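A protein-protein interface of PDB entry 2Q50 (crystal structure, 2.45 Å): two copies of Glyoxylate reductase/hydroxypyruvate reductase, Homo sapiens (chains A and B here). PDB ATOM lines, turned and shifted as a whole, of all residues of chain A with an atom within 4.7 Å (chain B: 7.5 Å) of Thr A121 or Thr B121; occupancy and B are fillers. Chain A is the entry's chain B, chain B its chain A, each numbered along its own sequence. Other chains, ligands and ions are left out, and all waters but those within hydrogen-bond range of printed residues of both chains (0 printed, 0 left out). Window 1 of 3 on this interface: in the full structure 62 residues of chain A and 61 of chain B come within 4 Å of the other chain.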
ATOM      1  N   SER A 117      10.261  19.482  15.238  1.00  0.00           N
ATOM      2  CA  SER A 117      10.945  20.760  15.031  1.00  0.00           C
ATOM      3  C   SER A 117      12.235  20.506  14.254  1.00  0.00           C
ATOM      4  O   SER A 117      12.603  21.268  13.357  1.00  0.00           O
ATOM      5  CB  SER A 117      11.285  21.424  16.369  1.00  0.00           C
ATOM      6  OG  SER A 117      10.114  21.718  17.104  1.00  0.00           O
ATOM      7  N   LEU A 118      12.920  19.424  14.605  1.00  0.00           N
ATOM      8  CA  LEU A 118      14.160  19.076  13.933  1.00  0.00           C
ATOM      9  C   LEU A 118      13.882  18.701  12.483  1.00  0.00           C
ATOM     10  O   LEU A 118      14.592  19.129  11.578  1.00  0.00           O
ATOM     11  CB  LEU A 118      14.850  17.915  14.652  1.00  0.00           C
ATOM     12  CG  LEU A 118      16.183  17.478  14.042  1.00  0.00           C
ATOM     13  CD1 LEU A 118      17.159  18.646  13.994  1.00  0.00           C
ATOM     14  CD2 LEU A 118      16.750  16.341  14.864  1.00  0.00           C
ATOM     15  N   LEU A 119      12.836  17.911  12.267  1.00  0.00           N
ATOM     16  CA  LEU A 119      12.465  17.482  10.926  1.00  0.00           C
ATOM     17  C   LEU A 119      12.175  18.701  10.046  1.00  0.00           C
ATOM     18  O   LEU A 119      12.720  18.840   8.953  1.00  0.00           O
ATOM     19  CB  LEU A 119      11.241  16.548  10.995  1.00  0.00           C
ATOM     20  CG  LEU A 119      10.637  16.007   9.685  1.00  0.00           C
ATOM     21  CD1 LEU A 119       9.800  14.767   9.981  1.00  0.00           C
ATOM     22  CD2 LEU A 119       9.783  17.064   9.002  1.00  0.00           C
ATOM     23  N   LEU A 120      11.325  19.592  10.532  1.00  0.00           N
ATOM     24  CA  LEU A 120      10.977  20.784   9.774  1.00  0.00           C
ATOM     25  C   LEU A 120      12.157  21.724   9.586  1.00  0.00           C
ATOM     26  O   LEU A 120      12.366  22.248   8.497  1.00  0.00           O
ATOM     27  CB  LEU A 120       9.818  21.515  10.456  1.00  0.00           C
ATOM     28  CG  LEU A 120       8.496  20.740  10.374  1.00  0.00           C
ATOM     29  CD1 LEU A 120       7.408  21.473  11.155  1.00  0.00           C
ATOM     30  CD2 LEU A 120       8.093  20.575   8.910  1.00  0.00           C
ATOM     31  N   THR A 121      12.933  21.928  10.645  1.00  0.00           N
ATOM     32  CA  THR A 121      14.085  22.814  10.578  1.00  0.00           C
ATOM     33  C   THR A 121      15.070  22.328   9.526  1.00  0.00           C
ATOM     34  O   THR A 121      15.738  23.124   8.864  1.00  0.00           O
ATOM     35  CB  THR A 121      14.814  22.876  11.924  1.00  0.00           C
ATOM     36  OG1 THR A 121      13.887  23.244  12.951  1.00  0.00           O
ATOM     37  CG2 THR A 121      15.924  23.893  11.874  1.00  0.00           C
ATOM     38  N   THR A 122      15.149  21.007   9.381  1.00  0.00           N
ATOM     39  CA  THR A 122      16.057  20.381   8.431  1.00  0.00           C
ATOM     40  C   THR A 122      15.544  20.384   6.994  1.00  0.00           C
ATOM     41  O   THR A 122      16.213  20.887   6.091  1.00  0.00           O
ATOM     42  CB  THR A 122      16.369  18.914   8.849  1.00  0.00           C
ATOM     43  OG1 THR A 122      17.016  18.903  10.129  1.00  0.00           O
ATOM     44  CG2 THR A 122      17.281  18.241   7.833  1.00  0.00           C
ATOM     45  N   CYS A 123      14.357  19.834   6.769  1.00  0.00           N
ATOM     46  CA  CYS A 123      13.837  19.768   5.409  1.00  0.00           C
ATOM     47  C   CYS A 123      13.476  21.135   4.830  1.00  0.00           C
ATOM     48  O   CYS A 123      13.416  21.300   3.608  1.00  0.00           O
ATOM     49  CB  CYS A 123      12.631  18.828   5.343  1.00  0.00           C
ATOM     50  SG  CYS A 123      11.119  19.511   6.014  1.00  0.00           S
ATOM     51  N   ARG A 124      13.234  22.116   5.694  1.00  0.00           N
ATOM     52  CA  ARG A 124      12.915  23.449   5.203  1.00  0.00           C
ATOM     53  C   ARG A 124      14.166  24.332   5.190  1.00  0.00           C
ATOM     54  O   ARG A 124      14.096  25.530   4.918  1.00  0.00           O
ATOM     55  CB  ARG A 124      11.787  24.086   6.027  1.00  0.00           C
ATOM     56  CG  ARG A 124      10.441  23.356   5.886  1.00  0.00           C
ATOM     57  CD  ARG A 124      10.058  23.147   4.418  1.00  0.00           C
ATOM     58  NE  ARG A 124      10.035  24.411   3.681  1.00  0.00           N
ATOM     59  CZ  ARG A 124       8.961  25.177   3.517  1.00  0.00           C
ATOM     60  NH1 ARG A 124       7.793  24.814   4.029  1.00  0.00           N
ATOM     61  NH2 ARG A 124       9.068  26.325   2.860  1.00  0.00           N
ATOM     62  N   ARG A 125      15.306  23.710   5.484  1.00  0.00           N
ATOM     63  CA  ARG A 125      16.618  24.364   5.469  1.00  0.00           C
ATOM     64  C   ARG A 125      16.704  25.658   6.256  1.00  0.00           C
ATOM     65  O   ARG A 125      17.439  26.582   5.887  1.00  0.00           O
ATOM     66  CB  ARG A 125      17.030  24.621   4.015  1.00  0.00           C
ATOM     67  CG  ARG A 125      16.891  23.391   3.132  1.00  0.00           C
ATOM     68  CD  ARG A 125      17.067  23.732   1.661  1.00  0.00           C
ATOM     69  NE  ARG A 125      18.440  24.110   1.341  1.00  0.00           N
ATOM     70  CZ  ARG A 125      18.857  24.455   0.124  1.00  0.00           C
ATOM     71  NH1 ARG A 125      18.008  24.470  -0.895  1.00  0.00           N
ATOM     72  NH2 ARG A 125      20.125  24.793  -0.069  1.00  0.00           N
ATOM     73  N   LEU A 126      15.969  25.733   7.354  1.00  0.00           N
ATOM     74  CA  LEU A 126      16.007  26.949   8.150  1.00  0.00           C
ATOM     75  C   LEU A 126      17.422  27.394   8.542  1.00  0.00           C
ATOM     76  O   LEU A 126      17.760  28.563   8.419  1.00  0.00           O
ATOM     77  CB  LEU A 126      15.114  26.796   9.379  1.00  0.00           C
ATOM     78  CG  LEU A 126      13.797  27.570   9.219  1.00  0.00           C
ATOM     79  CD1 LEU A 126      13.159  27.210   7.883  1.00  0.00           C
ATOM     80  CD2 LEU A 126      12.855  27.278  10.385  1.00  0.00           C
ATOM     81  N   PRO A 127      18.274  26.465   8.994  1.00  0.00           N
ATOM     82  CA  PRO A 127      19.627  26.896   9.369  1.00  0.00           C
ATOM     83  C   PRO A 127      20.336  27.677   8.264  1.00  0.00           C
ATOM     84  O   PRO A 127      20.823  28.785   8.489  1.00  0.00           O
ATOM     85  CB  PRO A 127      20.324  25.583   9.702  1.00  0.00           C
ATOM     86  CG  PRO A 127      19.189  24.762  10.267  1.00  0.00           C
ATOM     87  CD  PRO A 127      18.071  25.036   9.290  1.00  0.00           C
ATOM     88  N   LEU B 114       5.946  26.269   6.739  1.00  0.00           N
ATOM     89  CA  LEU B 114       7.118  27.022   7.128  1.00  0.00           C
ATOM     90  C   LEU B 114       6.825  27.834   8.385  1.00  0.00           C
ATOM     91  O   LEU B 114       7.682  27.990   9.257  1.00  0.00           O
ATOM     92  CB  LEU B 114       7.558  27.951   5.995  1.00  0.00           C
ATOM     93  CG  LEU B 114       8.883  28.613   6.347  1.00  0.00           C
ATOM     94  CD1 LEU B 114       9.973  27.562   6.464  1.00  0.00           C
ATOM     95  CD2 LEU B 114       9.217  29.624   5.309  1.00  0.00           C
ATOM     96  N   ALA B 115       5.603  28.351   8.476  1.00  0.00           N
ATOM     97  CA  ALA B 115       5.204  29.142   9.633  1.00  0.00           C
ATOM     98  C   ALA B 115       5.354  28.297  10.900  1.00  0.00           C
ATOM     99  O   ALA B 115       5.900  28.758  11.913  1.00  0.00           O
ATOM    100  CB  ALA B 115       3.765  29.629   9.471  1.00  0.00           C
ATOM    101  N   VAL B 116       4.891  27.052  10.841  1.00  0.00           N
ATOM    102  CA  VAL B 116       5.014  26.176  12.004  1.00  0.00           C
ATOM    103  C   VAL B 116       6.491  25.898  12.277  1.00  0.00           C
ATOM    104  O   VAL B 116       6.925  25.929  13.426  1.00  0.00           O
ATOM    105  CB  VAL B 116       4.263  24.849  11.795  1.00  0.00           C
ATOM    106  CG1 VAL B 116       4.481  23.927  12.997  1.00  0.00           C
ATOM    107  CG2 VAL B 116       2.769  25.130  11.598  1.00  0.00           C
ATOM    108  N   SER B 117       7.255  25.648  11.214  1.00  0.00           N
ATOM    109  CA  SER B 117       8.693  25.393  11.324  1.00  0.00           C
ATOM    110  C   SER B 117       9.363  26.559  12.040  1.00  0.00           C
ATOM    111  O   SER B 117      10.113  26.369  12.999  1.00  0.00           O
ATOM    112  CB  SER B 117       9.321  25.234   9.936  1.00  0.00           C
ATOM    113  OG  SER B 117       8.713  24.178   9.218  1.00  0.00           O
ATOM    114  N   LEU B 118       9.086  27.769  11.564  1.00  0.00           N
ATOM    115  CA  LEU B 118       9.645  28.972  12.170  1.00  0.00           C
ATOM    116  C   LEU B 118       9.239  29.090  13.649  1.00  0.00           C
ATOM    117  O   LEU B 118      10.049  29.451  14.502  1.00  0.00           O
ATOM    118  CB  LEU B 118       9.181  30.204  11.391  1.00  0.00           C
ATOM    119  CG  LEU B 118       9.656  31.576  11.870  1.00  0.00           C
ATOM    120  CD1 LEU B 118      11.154  31.590  12.035  1.00  0.00           C
ATOM    121  CD2 LEU B 118       9.229  32.624  10.872  1.00  0.00           C
ATOM    122  N   LEU B 119       7.990  28.764  13.953  1.00  0.00           N
ATOM    123  CA  LEU B 119       7.515  28.838  15.331  1.00  0.00           C
ATOM    124  C   LEU B 119       8.246  27.845  16.243  1.00  0.00           C
ATOM    125  O   LEU B 119       8.598  28.170  17.384  1.00  0.00           O
ATOM    126  CB  LEU B 119       5.996  28.591  15.385  1.00  0.00           C
ATOM    127  CG  LEU B 119       5.314  28.554  16.764  1.00  0.00           C
ATOM    128  CD1 LEU B 119       3.816  28.818  16.625  1.00  0.00           C
ATOM    129  CD2 LEU B 119       5.573  27.211  17.432  1.00  0.00           C
ATOM    130  N   LEU B 120       8.482  26.640  15.739  1.00  0.00           N
ATOM    131  CA  LEU B 120       9.152  25.622  16.534  1.00  0.00           C
ATOM    132  C   LEU B 120      10.644  25.852  16.771  1.00  0.00           C
ATOM    133  O   LEU B 120      11.134  25.590  17.870  1.00  0.00           O
ATOM    134  CB  LEU B 120       8.936  24.239  15.911  1.00  0.00           C
ATOM    135  CG  LEU B 120       7.519  23.660  15.991  1.00  0.00           C
ATOM    136  CD1 LEU B 120       7.522  22.260  15.404  1.00  0.00           C
ATOM    137  CD2 LEU B 120       7.044  23.624  17.439  1.00  0.00           C
ATOM    138  N   THR B 121      11.369  26.330  15.757  1.00  0.00           N
ATOM    139  CA  THR B 121      12.803  26.565  15.923  1.00  0.00           C
ATOM    140  C   THR B 121      13.034  27.688  16.922  1.00  0.00           C
ATOM    141  O   THR B 121      14.055  27.722  17.607  1.00  0.00           O
ATOM    142  CB  THR B 121      13.509  26.958  14.600  1.00  0.00           C
ATOM    143  OG1 THR B 121      13.012  28.220  14.140  1.00  0.00           O
ATOM    144  CG2 THR B 121      13.283  25.913  13.545  1.00  0.00           C
ATOM    145  N   THR B 122      12.075  28.603  17.002  1.00  0.00           N
ATOM    146  CA  THR B 122      12.173  29.727  17.916  1.00  0.00           C
ATOM    147  C   THR B 122      11.856  29.289  19.345  1.00  0.00           C
ATOM    148  O   THR B 122      12.706  29.389  20.237  1.00  0.00           O
ATOM    149  CB  THR B 122      11.205  30.862  17.501  1.00  0.00           C
ATOM    150  OG1 THR B 122      11.383  31.149  16.106  1.00  0.00           O
ATOM    151  CG2 THR B 122      11.478  32.133  18.315  1.00  0.00           C
ATOM    152  N   CYS B 123      10.646  28.786  19.563  1.00  0.00           N
ATOM    153  CA  CYS B 123      10.258  28.372  20.908  1.00  0.00           C
ATOM    154  C   CYS B 123      11.172  27.284  21.485  1.00  0.00           C
ATOM    155  O   CYS B 123      11.531  27.342  22.660  1.00  0.00           O
ATOM    156  CB  CYS B 123       8.796  27.913  20.929  1.00  0.00           C
ATOM    157  SG  CYS B 123       8.491  26.291  20.224  1.00  0.00           S
ATOM    158  N   ARG B 124      11.548  26.300  20.672  1.00  0.00           N
ATOM    159  CA  ARG B 124      12.441  25.241  21.136  1.00  0.00           C
ATOM    160  C   ARG B 124      13.922  25.639  20.982  1.00  0.00           C
ATOM    161  O   ARG B 124      14.829  24.838  21.221  1.00  0.00           O
ATOM    162  CB  ARG B 124      12.134  23.927  20.405  1.00  0.00           C
ATOM    163  CG  ARG B 124      10.754  23.348  20.754  1.00  0.00           C
ATOM    164  CD  ARG B 124      10.560  23.210  22.275  1.00  0.00           C
ATOM    165  NE  ARG B 124      11.521  22.281  22.866  1.00  0.00           N
ATOM    166  CZ  ARG B 124      11.335  20.970  22.979  1.00  0.00           C
ATOM    167  NH1 ARG B 124      10.213  20.414  22.553  1.00  0.00           N
ATOM    168  NH2 ARG B 124      12.287  20.212  23.497  1.00  0.00           N
ATOM    169  N   ARG B 125      14.141  26.886  20.567  1.00  0.00           N
ATOM    170  CA  ARG B 125      15.477  27.476  20.426  1.00  0.00           C
ATOM    171  C   ARG B 125      16.556  26.694  19.658  1.00  0.00           C
ATOM    172  O   ARG B 125      17.705  26.620  20.111  1.00  0.00           O
ATOM    173  CB  ARG B 125      16.005  27.802  21.825  1.00  0.00           C
ATOM    174  CG  ARG B 125      14.981  28.500  22.715  1.00  0.00           C
ATOM    175  CD  ARG B 125      15.404  28.488  24.165  1.00  0.00           C
ATOM    176  NE  ARG B 125      16.675  29.172  24.347  1.00  0.00           N
ATOM    177  CZ  ARG B 125      17.348  29.200  25.490  1.00  0.00           C
ATOM    178  NH1 ARG B 125      16.866  28.577  26.561  1.00  0.00           N
ATOM    179  NH2 ARG B 125      18.505  29.844  25.564  1.00  0.00           N
ATOM    180  N   LEU B 126      16.208  26.135  18.501  1.00  0.00           N
ATOM    181  CA  LEU B 126      17.179  25.378  17.711  1.00  0.00           C
ATOM    182  C   LEU B 126      18.408  26.194  17.290  1.00  0.00           C
ATOM    183  O   LEU B 126      19.545  25.741  17.461  1.00  0.00           O
ATOM    184  CB  LEU B 126      16.503  24.750  16.484  1.00  0.00           C
ATOM    185  CG  LEU B 126      15.928  23.340  16.716  1.00  0.00           C
ATOM    186  CD1 LEU B 126      15.025  23.326  17.942  1.00  0.00           C
ATOM    187  CD2 LEU B 126      15.169  22.894  15.487  1.00  0.00           C
ATOM    188  N   PRO B 127      18.203  27.413  16.751  1.00  0.00           N
ATOM    189  CA  PRO B 127      19.338  28.245  16.330  1.00  0.00           C
ATOM    190  C   PRO B 127      20.438  28.353  17.399  1.00  0.00           C
ATOM    191  O   PRO B 127      21.612  28.119  17.104  1.00  0.00           O
ATOM    192  CB  PRO B 127      18.685  29.591  16.028  1.00  0.00           C
ATOM    193  CG  PRO B 127      17.332  29.196  15.537  1.00  0.00           C
ATOM    194  CD  PRO B 127      16.928  28.111  16.509  1.00  0.00           C
ATOM    195  N   GLU B 128      20.058  28.701  18.633  1.00  0.00           N
ATOM    196  CA  GLU B 128      21.028  28.817  19.727  1.00  0.00           C
ATOM    197  C   GLU B 128      21.729  27.483  19.959  1.00  0.00           C
ATOM    198  O   GLU B 128      22.955  27.423  20.077  1.00  0.00           O
ATOM    199  CB  GLU B 128      20.350  29.233  21.042  1.00  0.00           C
ATOM    200  CG  GLU B 128      19.652  30.591  21.030  1.00  0.00           C
ATOM    201  CD  GLU B 128      18.994  30.928  22.366  1.00  0.00           C
ATOM    202  OE1 GLU B 128      19.724  31.201  23.345  1.00  0.00           O
ATOM    203  OE2 GLU B 128      17.746  30.912  22.437  1.00  0.00           O
ATOM    204  N   ALA B 129      20.938  26.417  20.035  1.00  0.00           N
ATOM    205  CA  ALA B 129      21.474  25.083  20.273  1.00  0.00           C
ATOM    206  C   ALA B 129      22.509  24.712  19.217  1.00  0.00           C
ATOM    207  O   ALA B 129      23.638  24.333  19.552  1.00  0.00           O
ATOM    208  CB  ALA B 129      20.338  24.065  20.296  1.00  0.00           C
ATOM    209  N   ILE B 130      22.121  24.828  17.946  1.00  0.00           N
ATOM    210  CA  ILE B 130      23.016  24.519  16.827  1.00  0.00           C
ATOM    211  C   ILE B 130      24.368  25.204  17.012  1.00  0.00           C
ATOM    212  O   ILE B 130      25.419  24.602  16.792  1.00  0.00           O
ATOM    213  CB  ILE B 130      22.423  24.998  15.491  1.00  0.00           C
ATOM    214  CG1 ILE B 130      21.146  24.210  15.185  1.00  0.00           C
ATOM    215  CG2 ILE B 130      23.454  24.849  14.377  1.00  0.00           C
ATOM    216  CD1 ILE B 130      20.381  24.711  13.974  1.00  0.00           C
ATOM    217  N   ILE B 241       5.531  35.436  16.097  1.00  0.00           N
ATOM    218  CA  ILE B 241       5.934  34.960  14.771  1.00  0.00           C
ATOM    219  C   ILE B 241       5.246  35.777  13.672  1.00  0.00           C
ATOM    220  O   ILE B 241       4.058  36.083  13.770  1.00  0.00           O
ATOM    221  CB  ILE B 241       5.541  33.461  14.559  1.00  0.00           C
ATOM    222  CG1 ILE B 241       6.114  32.586  15.683  1.00  0.00           C
ATOM    223  CG2 ILE B 241       6.019  32.975  13.193  1.00  0.00           C
ATOM    224  CD1 ILE B 241       7.605  32.745  15.915  1.00  0.00           C
ATOM    225  N   GLY B 267      10.275  35.261  15.726  1.00  0.00           N
ATOM    226  CA  GLY B 267      10.714  34.605  14.514  1.00  0.00           C
ATOM    227  C   GLY B 267      10.013  35.268  13.344  1.00  0.00           C
ATOM    228  O   GLY B 267       8.780  35.320  13.289  1.00  0.00           O
ATOM    229  N   VAL B 289      14.816  35.301  15.221  1.00  0.00           N
ATOM    230  CA  VAL B 289      14.881  34.248  14.213  1.00  0.00           C
ATOM    231  C   VAL B 289      14.352  34.811  12.902  1.00  0.00           C
ATOM    232  O   VAL B 289      13.150  34.780  12.640  1.00  0.00           O
ATOM    233  CB  VAL B 289      14.024  33.018  14.618  1.00  0.00           C
ATOM    234  CG1 VAL B 289      13.991  32.014  13.485  1.00  0.00           C
ATOM    235  CG2 VAL B 289      14.591  32.366  15.868  1.00  0.00           C
ATOM    236  N   LEU B 291      14.178  34.761   8.781  1.00  0.00           N
ATOM    237  CA  LEU B 291      14.373  33.943   7.594  1.00  0.00           C
ATOM    238  C   LEU B 291      14.236  34.883   6.409  1.00  0.00           C
ATOM    239  O   LEU B 291      13.527  35.890   6.488  1.00  0.00           O
ATOM    240  CB  LEU B 291      13.313  32.835   7.519  1.00  0.00           C
ATOM    241  CG  LEU B 291      13.173  31.909   8.742  1.00  0.00           C
ATOM    242  CD1 LEU B 291      12.051  30.904   8.499  1.00  0.00           C
ATOM    243  CD2 LEU B 291      14.489  31.199   9.017  1.00  0.00           C
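The backbone carbonyl oxygen (O) of Leu B118 lies within hydrogen-bond range of the side-chain hydroxyl (OG1) of Thr B121. The backbone carbonyl oxygen of Leu B118 sits at hydrogen-bond distance from the side-chain hydroxyl of Thr B122 (2.7 Å). SG of Cys B123 is in hydrogen-bond range of O of Leu B120, at 3.6 Å. N of Leu B126 sits at hydrogen-bond distance from O of Thr B121 (2.8 Å). The backbone carbonyl oxygen (O) of Thr A121 sits at hydrogen-bond distance from the backbone NH (N) of Leu A126, 3.0 Å away.
Ser A117 touches Leu B120 (OG to CB, 3.0 Å). CD2 of Leu B126 touches O of Ser A117, 3.7 Å away. Leu A120 touches Ser B117 (CB to OG, 3.1 Å). Thr A121 touches Thr B121. Arg A124 touches Leu B114. Ser B117 touches Arg A124 (OG to CG, 3.8 Å). CD1 of Leu B114 touches CD1 of Leu A126, at 3.5 Å. CD2 of Leu A126 touches N of Leu B118 (3.98 Å). Leu A126 touches Thr B121 (CD2 to CG2, 3.5 Å). Pro A127 touches Ile B130 (CG to CD1, 3.9 Å).
Printed residues of chain B within 4 Å of Ser A117: Leu B120 and Leu B126. Leu A118 touches none of the printed residues of chain B. Of the printed residues of chain B, Arg A124 touches Leu B114 (3.6 Å) and Ser B117 (3.8 Å). Of the printed residues of chain A, Leu B114 touches Arg A124 and Leu A126. Printed residues of chain A within 4 Å of Ser B117: Leu A120 (3.1 Å), Arg A124 (3.8 Å) and Leu A126 (3.9 Å). The nearest residue of chain B that does not touch Thr A121 is Ser B117 (4.9 Å). The nearest printed residue of chain A that does not touch Thr B121 is Ser A117 (4.7 Å). The nearest printed residue of chain B that does not touch Pro A127 is Leu B291 (6.1 Å).
Printed residues of chain A that touch a printed residue of chain B: Ser A117, Leu A120, Thr A121, Arg A124, Leu A126 and Pro A127. Among the printed residues, 13 pairs touch across the chains. Among the printed residues, no Asp or Glu carboxylate lies within 4 Å of a Lys or Arg side-chain nitrogen of the other chain.
Ser A117 touches Leu B126, and with the chains exchanged Leu A126 touches Ser B117. Thr B121 touches its own counterpart, Thr A121. Thr A121 touches Leu B126, and with the chains exchanged Leu A126 touches Thr B121. Arg A124 touches Ser B117, but with the chains exchanged Ser A117 does not touch Arg B124 (4.05 Å). Positions printed for both chains: 117, 118, 119, 120, 121, 122, 123, 124, 125, 126 and 127. Of the 13 pairs that touch across the chains among the printed residues, 7 have their exchanged pair printed and touching as well.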
